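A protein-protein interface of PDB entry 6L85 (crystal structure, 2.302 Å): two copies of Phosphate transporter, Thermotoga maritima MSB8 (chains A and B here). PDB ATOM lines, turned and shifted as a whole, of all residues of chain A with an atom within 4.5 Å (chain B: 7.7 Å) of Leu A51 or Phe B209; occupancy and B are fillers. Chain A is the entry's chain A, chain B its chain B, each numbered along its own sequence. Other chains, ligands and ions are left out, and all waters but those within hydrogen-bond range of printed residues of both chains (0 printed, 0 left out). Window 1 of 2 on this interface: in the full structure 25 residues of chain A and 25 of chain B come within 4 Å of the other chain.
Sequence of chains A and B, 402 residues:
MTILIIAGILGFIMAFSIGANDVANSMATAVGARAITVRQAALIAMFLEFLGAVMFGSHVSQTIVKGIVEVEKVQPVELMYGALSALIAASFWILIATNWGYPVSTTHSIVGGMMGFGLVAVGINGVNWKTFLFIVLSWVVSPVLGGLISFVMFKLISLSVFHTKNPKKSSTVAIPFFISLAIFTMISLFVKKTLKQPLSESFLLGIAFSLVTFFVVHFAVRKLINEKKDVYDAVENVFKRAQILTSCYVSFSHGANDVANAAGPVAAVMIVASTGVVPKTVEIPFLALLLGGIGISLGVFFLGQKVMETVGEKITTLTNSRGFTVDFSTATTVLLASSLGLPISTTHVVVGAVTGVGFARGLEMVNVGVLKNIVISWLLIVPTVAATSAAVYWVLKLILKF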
ATOM      1  N   PHE A  47      13.557  -0.753  19.623  1.00  0.00           N
ATOM      2  CA  PHE A  47      13.545  -0.760  21.078  1.00  0.00           C
ATOM      3  C   PHE A  47      14.261   0.467  21.663  1.00  0.00           C
ATOM      4  O   PHE A  47      13.736   1.135  22.567  1.00  0.00           O
ATOM      5  CB  PHE A  47      14.141  -2.057  21.607  1.00  0.00           C
ATOM      6  CG  PHE A  47      13.504  -2.495  22.857  1.00  0.00           C
ATOM      7  CD1 PHE A  47      13.859  -1.910  24.055  1.00  0.00           C
ATOM      8  CD2 PHE A  47      12.504  -3.446  22.840  1.00  0.00           C
ATOM      9  CE1 PHE A  47      13.245  -2.284  25.228  1.00  0.00           C
ATOM     10  CE2 PHE A  47      11.896  -3.832  23.997  1.00  0.00           C
ATOM     11  CZ  PHE A  47      12.261  -3.250  25.200  1.00  0.00           C
ATOM     12  N   LEU A  48      15.445   0.792  21.146  1.00  0.00           N
ATOM     13  CA  LEU A  48      16.261   1.832  21.781  1.00  0.00           C
ATOM     14  C   LEU A  48      15.691   3.236  21.554  1.00  0.00           C
ATOM     15  O   LEU A  48      15.790   4.087  22.447  1.00  0.00           O
ATOM     16  CB  LEU A  48      17.710   1.744  21.301  1.00  0.00           C
ATOM     17  CG  LEU A  48      18.686   0.797  22.051  1.00  0.00           C
ATOM     18  CD1 LEU A  48      18.998   1.266  23.471  1.00  0.00           C
ATOM     19  CD2 LEU A  48      18.194  -0.654  22.074  1.00  0.00           C
ATOM     20  N   GLU A  49      15.066   3.494  20.397  1.00  0.00           N
ATOM     21  CA  GLU A  49      14.400   4.777  20.185  1.00  0.00           C
ATOM     22  C   GLU A  49      13.300   4.972  21.212  1.00  0.00           C
ATOM     23  O   GLU A  49      13.194   6.038  21.831  1.00  0.00           O
ATOM     24  CB  GLU A  49      13.798   4.867  18.777  1.00  0.00           C
ATOM     25  CG  GLU A  49      14.775   4.718  17.641  1.00  0.00           C
ATOM     26  CD  GLU A  49      15.406   6.023  17.269  1.00  0.00           C
ATOM     27  OE1 GLU A  49      14.907   7.053  17.762  1.00  0.00           O
ATOM     28  OE2 GLU A  49      16.385   6.012  16.490  1.00  0.00           O
ATOM     29  N   PHE A  50      12.448   3.954  21.374  1.00  0.00           N
ATOM     30  CA  PHE A  50      11.342   4.045  22.325  1.00  0.00           C
ATOM     31  C   PHE A  50      11.869   4.274  23.735  1.00  0.00           C
ATOM     32  O   PHE A  50      11.332   5.102  24.482  1.00  0.00           O
ATOM     33  CB  PHE A  50      10.479   2.776  22.232  1.00  0.00           C
ATOM     34  CG  PHE A  50       9.404   2.678  23.296  1.00  0.00           C
ATOM     35  CD1 PHE A  50       8.181   3.309  23.130  1.00  0.00           C
ATOM     36  CD2 PHE A  50       9.630   1.969  24.463  1.00  0.00           C
ATOM     37  CE1 PHE A  50       7.200   3.245  24.117  1.00  0.00           C
ATOM     38  CE2 PHE A  50       8.638   1.884  25.448  1.00  0.00           C
ATOM     39  CZ  PHE A  50       7.428   2.525  25.268  1.00  0.00           C
ATOM     40  N   LEU A  51      12.960   3.587  24.091  1.00  0.00           N
ATOM     41  CA  LEU A  51      13.527   3.709  25.432  1.00  0.00           C
ATOM     42  C   LEU A  51      14.082   5.113  25.692  1.00  0.00           C
ATOM     43  O   LEU A  51      13.874   5.677  26.774  1.00  0.00           O
ATOM     44  CB  LEU A  51      14.621   2.658  25.613  1.00  0.00           C
ATOM     45  CG  LEU A  51      15.196   2.495  27.015  1.00  0.00           C
ATOM     46  CD1 LEU A  51      14.156   1.860  27.952  1.00  0.00           C
ATOM     47  CD2 LEU A  51      16.481   1.677  26.971  1.00  0.00           C
ATOM     48  N   GLY A  52      14.813   5.680  24.718  1.00  0.00           N
ATOM     49  CA  GLY A  52      15.276   7.054  24.864  1.00  0.00           C
ATOM     50  C   GLY A  52      14.129   8.041  24.971  1.00  0.00           C
ATOM     51  O   GLY A  52      14.158   8.959  25.796  1.00  0.00           O
ATOM     52  N   ALA A  53      13.096   7.850  24.148  1.00  0.00           N
ATOM     53  CA  ALA A  53      11.923   8.712  24.190  1.00  0.00           C
ATOM     54  C   ALA A  53      11.269   8.713  25.570  1.00  0.00           C
ATOM     55  O   ALA A  53      10.857   9.774  26.066  1.00  0.00           O
ATOM     56  CB  ALA A  53      10.911   8.265  23.129  1.00  0.00           C
ATOM     57  N   VAL A  54      11.153   7.530  26.199  1.00  0.00           N
ATOM     58  CA  VAL A  54      10.475   7.424  27.497  1.00  0.00           C
ATOM     59  C   VAL A  54      11.376   7.905  28.635  1.00  0.00           C
ATOM     60  O   VAL A  54      10.935   8.627  29.536  1.00  0.00           O
ATOM     61  CB  VAL A  54      10.006   5.970  27.746  1.00  0.00           C
ATOM     62  CG1 VAL A  54       9.658   5.772  29.206  1.00  0.00           C
ATOM     63  CG2 VAL A  54       8.811   5.642  26.886  1.00  0.00           C
ATOM     64  N   MET A  55      12.637   7.479  28.649  1.00  0.00           N
ATOM     65  CA  MET A  55      13.507   7.819  29.767  1.00  0.00           C
ATOM     66  C   MET A  55      13.917   9.290  29.748  1.00  0.00           C
ATOM     67  O   MET A  55      14.172   9.871  30.813  1.00  0.00           O
ATOM     68  CB  MET A  55      14.759   6.925  29.762  1.00  0.00           C
ATOM     69  CG  MET A  55      14.449   5.434  29.954  1.00  0.00           C
ATOM     70  SD  MET A  55      15.866   4.346  30.274  1.00  0.00           S
ATOM     71  CE  MET A  55      16.795   5.261  31.497  1.00  0.00           C
ATOM     72  N   PHE A 252      19.147   5.508  21.206  1.00  0.00           N
ATOM     73  CA  PHE A 252      18.608   6.025  22.464  1.00  0.00           C
ATOM     74  C   PHE A 252      18.635   7.554  22.488  1.00  0.00           C
ATOM     75  O   PHE A 252      17.636   8.207  22.843  1.00  0.00           O
ATOM     76  CB  PHE A 252      19.417   5.458  23.642  1.00  0.00           C
ATOM     77  CG  PHE A 252      18.949   5.934  25.012  1.00  0.00           C
ATOM     78  CD1 PHE A 252      19.418   7.136  25.558  1.00  0.00           C
ATOM     79  CD2 PHE A 252      18.104   5.138  25.788  1.00  0.00           C
ATOM     80  CE1 PHE A 252      19.010   7.558  26.830  1.00  0.00           C
ATOM     81  CE2 PHE A 252      17.680   5.550  27.056  1.00  0.00           C
ATOM     82  CZ  PHE A 252      18.132   6.762  27.578  1.00  0.00           C
ATOM     83  N   ILE B 179       7.060 -13.008  26.996  1.00  0.00           N
ATOM     84  CA  ILE B 179       8.124 -12.009  27.160  1.00  0.00           C
ATOM     85  C   ILE B 179       7.520 -10.636  27.462  1.00  0.00           C
ATOM     86  O   ILE B 179       7.987  -9.914  28.362  1.00  0.00           O
ATOM     87  CB  ILE B 179       9.021 -11.965  25.911  1.00  0.00           C
ATOM     88  CG1 ILE B 179       9.571 -13.351  25.610  1.00  0.00           C
ATOM     89  CG2 ILE B 179      10.196 -11.012  26.112  1.00  0.00           C
ATOM     90  CD1 ILE B 179      10.422 -13.872  26.719  1.00  0.00           C
ATOM     91  N   SER B 180       6.446 -10.282  26.747  1.00  0.00           N
ATOM     92  CA  SER B 180       5.744  -9.020  26.959  1.00  0.00           C
ATOM     93  C   SER B 180       5.083  -8.948  28.325  1.00  0.00           C
ATOM     94  O   SER B 180       5.034  -7.878  28.942  1.00  0.00           O
ATOM     95  CB  SER B 180       4.693  -8.825  25.869  1.00  0.00           C
ATOM     96  OG  SER B 180       5.351  -8.753  24.629  1.00  0.00           O
ATOM     97  N   ILE B 183       7.900  -8.129  30.809  1.00  0.00           N
ATOM     98  CA  ILE B 183       8.252  -6.711  30.715  1.00  0.00           C
ATOM     99  C   ILE B 183       7.169  -5.832  31.340  1.00  0.00           C
ATOM    100  O   ILE B 183       7.469  -4.873  32.071  1.00  0.00           O
ATOM    101  CB  ILE B 183       8.507  -6.360  29.234  1.00  0.00           C
ATOM    102  CG1 ILE B 183       9.945  -6.699  28.875  1.00  0.00           C
ATOM    103  CG2 ILE B 183       8.232  -4.912  28.966  1.00  0.00           C
ATOM    104  CD1 ILE B 183      10.927  -5.750  29.554  1.00  0.00           C
ATOM    105  N   PHE B 184       5.892  -6.133  31.060  1.00  0.00           N
ATOM    106  CA  PHE B 184       4.806  -5.378  31.681  1.00  0.00           C
ATOM    107  C   PHE B 184       4.908  -5.428  33.197  1.00  0.00           C
ATOM    108  O   PHE B 184       4.715  -4.413  33.877  1.00  0.00           O
ATOM    109  CB  PHE B 184       3.430  -5.907  31.258  1.00  0.00           C
ATOM    110  CG  PHE B 184       2.300  -5.343  32.094  1.00  0.00           C
ATOM    111  CD1 PHE B 184       1.690  -4.157  31.739  1.00  0.00           C
ATOM    112  CD2 PHE B 184       1.877  -5.979  33.252  1.00  0.00           C
ATOM    113  CE1 PHE B 184       0.671  -3.622  32.502  1.00  0.00           C
ATOM    114  CE2 PHE B 184       0.871  -5.439  34.025  1.00  0.00           C
ATOM    115  CZ  PHE B 184       0.262  -4.259  33.644  1.00  0.00           C
ATOM    116  N   ILE B 187       8.062  -3.308  34.462  1.00  0.00           N
ATOM    117  CA  ILE B 187       7.912  -1.877  34.270  1.00  0.00           C
ATOM    118  C   ILE B 187       6.814  -1.324  35.170  1.00  0.00           C
ATOM    119  O   ILE B 187       7.015  -0.318  35.865  1.00  0.00           O
ATOM    120  CB  ILE B 187       7.641  -1.572  32.781  1.00  0.00           C
ATOM    121  CG1 ILE B 187       8.844  -1.970  31.918  1.00  0.00           C
ATOM    122  CG2 ILE B 187       7.247  -0.099  32.585  1.00  0.00           C
ATOM    123  CD1 ILE B 187      10.084  -1.213  32.228  1.00  0.00           C
ATOM    124  N   SER B 188       5.628  -1.946  35.160  1.00  0.00           N
ATOM    125  CA  SER B 188       4.537  -1.419  35.975  1.00  0.00           C
ATOM    126  C   SER B 188       4.913  -1.404  37.448  1.00  0.00           C
ATOM    127  O   SER B 188       4.641  -0.424  38.148  1.00  0.00           O
ATOM    128  CB  SER B 188       3.257  -2.223  35.741  1.00  0.00           C
ATOM    129  OG  SER B 188       3.444  -3.576  36.125  1.00  0.00           O
ATOM    130  N   VAL B 191       7.566   1.460  38.022  1.00  0.00           N
ATOM    131  CA  VAL B 191       6.989   2.791  37.949  1.00  0.00           C
ATOM    132  C   VAL B 191       6.071   3.034  39.142  1.00  0.00           C
ATOM    133  O   VAL B 191       6.047   4.133  39.710  1.00  0.00           O
ATOM    134  CB  VAL B 191       6.255   2.964  36.606  1.00  0.00           C
ATOM    135  CG1 VAL B 191       5.421   4.256  36.623  1.00  0.00           C
ATOM    136  CG2 VAL B 191       7.277   2.944  35.435  1.00  0.00           C
ATOM    137  N   SER B 202       1.502   3.958  35.737  1.00  0.00           N
ATOM    138  CA  SER B 202       2.271   2.720  35.799  1.00  0.00           C
ATOM    139  C   SER B 202       1.759   1.703  34.788  1.00  0.00           C
ATOM    140  O   SER B 202       2.545   1.095  34.050  1.00  0.00           O
ATOM    141  CB  SER B 202       2.213   2.147  37.207  1.00  0.00           C
ATOM    142  OG  SER B 202       2.769   3.078  38.111  1.00  0.00           O
ATOM    143  N   PHE B 203       0.439   1.513  34.737  1.00  0.00           N
ATOM    144  CA  PHE B 203      -0.132   0.552  33.798  1.00  0.00           C
ATOM    145  C   PHE B 203       0.076   1.002  32.366  1.00  0.00           C
ATOM    146  O   PHE B 203       0.347   0.184  31.486  1.00  0.00           O
ATOM    147  CB  PHE B 203      -1.628   0.358  34.066  1.00  0.00           C
ATOM    148  CG  PHE B 203      -1.926  -0.579  35.198  1.00  0.00           C
ATOM    149  CD1 PHE B 203      -1.084  -1.656  35.466  1.00  0.00           C
ATOM    150  CD2 PHE B 203      -3.055  -0.400  35.985  1.00  0.00           C
ATOM    151  CE1 PHE B 203      -1.362  -2.540  36.509  1.00  0.00           C
ATOM    152  CE2 PHE B 203      -3.344  -1.279  37.029  1.00  0.00           C
ATOM    153  CZ  PHE B 203      -2.491  -2.348  37.295  1.00  0.00           C
ATOM    154  N   LEU B 204      -0.078   2.301  32.106  1.00  0.00           N
ATOM    155  CA  LEU B 204       0.079   2.793  30.743  1.00  0.00           C
ATOM    156  C   LEU B 204       1.503   2.563  30.243  1.00  0.00           C
ATOM    157  O   LEU B 204       1.714   2.117  29.106  1.00  0.00           O
ATOM    158  CB  LEU B 204      -0.298   4.273  30.703  1.00  0.00           C
ATOM    159  CG  LEU B 204      -0.125   4.975  29.369  1.00  0.00           C
ATOM    160  CD1 LEU B 204      -1.183   4.482  28.400  1.00  0.00           C
ATOM    161  CD2 LEU B 204      -0.175   6.490  29.556  1.00  0.00           C
ATOM    162  N   LEU B 205       2.497   2.814  31.100  1.00  0.00           N
ATOM    163  CA  LEU B 205       3.882   2.557  30.710  1.00  0.00           C
ATOM    164  C   LEU B 205       4.148   1.060  30.563  1.00  0.00           C
ATOM    165  O   LEU B 205       4.854   0.633  29.633  1.00  0.00           O
ATOM    166  CB  LEU B 205       4.832   3.199  31.732  1.00  0.00           C
ATOM    167  CG  LEU B 205       4.995   4.707  31.491  1.00  0.00           C
ATOM    168  CD1 LEU B 205       5.522   5.439  32.716  1.00  0.00           C
ATOM    169  CD2 LEU B 205       5.928   4.912  30.311  1.00  0.00           C
ATOM    170  N   GLY B 206       3.611   0.243  31.482  1.00  0.00           N
ATOM    171  CA  GLY B 206       3.747  -1.200  31.330  1.00  0.00           C
ATOM    172  C   GLY B 206       3.197  -1.685  30.006  1.00  0.00           C
ATOM    173  O   GLY B 206       3.840  -2.473  29.305  1.00  0.00           O
ATOM    174  N   ILE B 207       2.013  -1.189  29.624  1.00  0.00           N
ATOM    175  CA  ILE B 207       1.395  -1.622  28.373  1.00  0.00           C
ATOM    176  C   ILE B 207       2.231  -1.183  27.181  1.00  0.00           C
ATOM    177  O   ILE B 207       2.443  -1.961  26.244  1.00  0.00           O
ATOM    178  CB  ILE B 207      -0.052  -1.100  28.267  1.00  0.00           C
ATOM    179  CG1 ILE B 207      -0.925  -1.670  29.385  1.00  0.00           C
ATOM    180  CG2 ILE B 207      -0.662  -1.516  26.936  1.00  0.00           C
ATOM    181  CD1 ILE B 207      -1.246  -3.144  29.181  1.00  0.00           C
ATOM    182  N   ALA B 208       2.718   0.066  27.174  1.00  0.00           N
ATOM    183  CA  ALA B 208       3.468   0.502  25.991  1.00  0.00           C
ATOM    184  C   ALA B 208       4.750  -0.316  25.824  1.00  0.00           C
ATOM    185  O   ALA B 208       5.099  -0.735  24.705  1.00  0.00           O
ATOM    186  CB  ALA B 208       3.767   2.000  26.070  1.00  0.00           C
ATOM    187  N   PHE B 209       5.470  -0.555  26.927  1.00  0.00           N
ATOM    188  CA  PHE B 209       6.654  -1.409  26.858  1.00  0.00           C
ATOM    189  C   PHE B 209       6.298  -2.811  26.366  1.00  0.00           C
ATOM    190  O   PHE B 209       7.061  -3.425  25.602  1.00  0.00           O
ATOM    191  CB  PHE B 209       7.322  -1.480  28.230  1.00  0.00           C
ATOM    192  CG  PHE B 209       8.332  -0.393  28.468  1.00  0.00           C
ATOM    193  CD1 PHE B 209       7.930   0.877  28.851  1.00  0.00           C
ATOM    194  CD2 PHE B 209       9.677  -0.638  28.297  1.00  0.00           C
ATOM    195  CE1 PHE B 209       8.861   1.885  29.065  1.00  0.00           C
ATOM    196  CE2 PHE B 209      10.610   0.369  28.508  1.00  0.00           C
ATOM    197  CZ  PHE B 209      10.200   1.626  28.895  1.00  0.00           C
ATOM    198  N   SER B 210       5.131  -3.328  26.792  1.00  0.00           N
ATOM    199  CA  SER B 210       4.668  -4.641  26.334  1.00  0.00           C
ATOM    200  C   SER B 210       4.455  -4.657  24.835  1.00  0.00           C
ATOM    201  O   SER B 210       4.796  -5.630  24.161  1.00  0.00           O
ATOM    202  CB  SER B 210       3.350  -5.013  27.016  1.00  0.00           C
ATOM    203  OG  SER B 210       3.577  -5.265  28.372  1.00  0.00           O
ATOM    204  N   LEU B 211       3.803  -3.617  24.314  1.00  0.00           N
ATOM    205  CA  LEU B 211       3.497  -3.553  22.888  1.00  0.00           C
ATOM    206  C   LEU B 211       4.767  -3.576  22.054  1.00  0.00           C
ATOM    207  O   LEU B 211       4.880  -4.354  21.089  1.00  0.00           O
ATOM    208  CB  LEU B 211       2.674  -2.297  22.596  1.00  0.00           C
ATOM    209  CG  LEU B 211       1.300  -2.493  23.230  1.00  0.00           C
ATOM    210  CD1 LEU B 211       0.454  -1.233  23.153  1.00  0.00           C
ATOM    211  CD2 LEU B 211       0.621  -3.671  22.519  1.00  0.00           C
ATOM    212  N   VAL B 212       5.752  -2.739  22.426  1.00  0.00           N
ATOM    213  CA  VAL B 212       7.015  -2.717  21.676  1.00  0.00           C
ATOM    214  C   VAL B 212       7.720  -4.067  21.772  1.00  0.00           C
ATOM    215  O   VAL B 212       8.239  -4.600  20.776  1.00  0.00           O
ATOM    216  CB  VAL B 212       7.928  -1.586  22.179  1.00  0.00           C
ATOM    217  CG1 VAL B 212       9.230  -1.586  21.382  1.00  0.00           C
ATOM    218  CG2 VAL B 212       7.208  -0.242  22.081  1.00  0.00           C
ATOM    219  N   THR B 213       7.775  -4.621  22.990  1.00  0.00           N
ATOM    220  CA  THR B 213       8.403  -5.918  23.217  1.00  0.00           C
ATOM    221  C   THR B 213       7.748  -7.002  22.370  1.00  0.00           C
ATOM    222  O   THR B 213       8.435  -7.793  21.715  1.00  0.00           O
ATOM    223  CB  THR B 213       8.312  -6.255  24.710  1.00  0.00           C
ATOM    224  OG1 THR B 213       8.953  -5.216  25.472  1.00  0.00           O
ATOM    225  CG2 THR B 213       8.958  -7.622  25.032  1.00  0.00           C
ATOM    226  N   PHE B 214       6.412  -7.043  22.363  1.00  0.00           N
ATOM    227  CA  PHE B 214       5.704  -8.062  21.597  1.00  0.00           C
ATOM    228  C   PHE B 214       6.049  -7.953  20.128  1.00  0.00           C
ATOM    229  O   PHE B 214       6.293  -8.968  19.467  1.00  0.00           O
ATOM    230  CB  PHE B 214       4.183  -7.945  21.797  1.00  0.00           C
ATOM    231  CG  PHE B 214       3.394  -9.078  21.151  1.00  0.00           C
ATOM    232  CD1 PHE B 214       3.180  -9.108  19.771  1.00  0.00           C
ATOM    233  CD2 PHE B 214       2.886 -10.118  21.921  1.00  0.00           C
ATOM    234  CE1 PHE B 214       2.477 -10.160  19.169  1.00  0.00           C
ATOM    235  CE2 PHE B 214       2.181 -11.176  21.331  1.00  0.00           C
ATOM    236  CZ  PHE B 214       1.976 -11.199  19.953  1.00  0.00           C
ATOM    237  N   PHE B 215       6.078  -6.724  19.600  1.00  0.00           N
ATOM    238  CA  PHE B 215       6.387  -6.536  18.185  1.00  0.00           C
ATOM    239  C   PHE B 215       7.771  -7.096  17.853  1.00  0.00           C
ATOM    240  O   PHE B 215       7.935  -7.930  16.939  1.00  0.00           O
ATOM    241  CB  PHE B 215       6.290  -5.044  17.849  1.00  0.00           C
ATOM    242  CG  PHE B 215       6.362  -4.737  16.378  1.00  0.00           C
ATOM    243  CD1 PHE B 215       7.573  -4.792  15.703  1.00  0.00           C
ATOM    244  CD2 PHE B 215       5.214  -4.399  15.668  1.00  0.00           C
ATOM    245  CE1 PHE B 215       7.645  -4.513  14.352  1.00  0.00           C
ATOM    246  CE2 PHE B 215       5.283  -4.115  14.318  1.00  0.00           C
ATOM    247  CZ  PHE B 215       6.504  -4.170  13.660  1.00  0.00           C
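OG1 of Thr B213 lies within hydrogen-bond range of O of Phe B209 (2.6 Å).
Among the printed residues, pairs that only touch across the chains: Phe A47 with Thr B213, Phe A50 with Phe B209, Phe A50 with Ala B208, Phe A50 with Val B212, Leu A51 with Phe B209, Val A54 with Phe B209 and Val A54 with Leu B205.
Leu A51 touches just one residue of chain B: Phe B209 (3.9 Å).
No residue of chain B comes within 4 Å of Gly A52.
Met A55 touches none of the printed residues of chain B.
Ser B180 touches none of the printed residues of chain A.
Printed residues of chain A within 4 Å of Leu B205: Val A54 (3.98 Å).
Of the printed residues of chain A, Thr B213 touches Phe A47.
The nearest residue of chain B that does not touch Leu A51 is Ile B187 (6.7 Å).
The nearest printed residue of chain A that does not touch Phe B209 is Phe A47 (4.8 Å).
The nearest printed residue of chain A that does not touch Thr B213 is Phe A50 (7.0 Å).
Of the 21 printed residues of chain B, 5 touch a printed residue of chain A.
Along chain B the printed residues that touch a printed residue of chain A span positions 205 to 213.
Of the 10 printed residues of chain A, 4 touch a printed residue of chain B.
Along chain A the printed residues that touch a printed residue of chain B span positions 47 to 54.
Among the printed residues, no Asp or Glu carboxylate lies within 4 Å of a Lys or Arg side-chain nitrogen of the other chain.
No position is printed for both chains.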
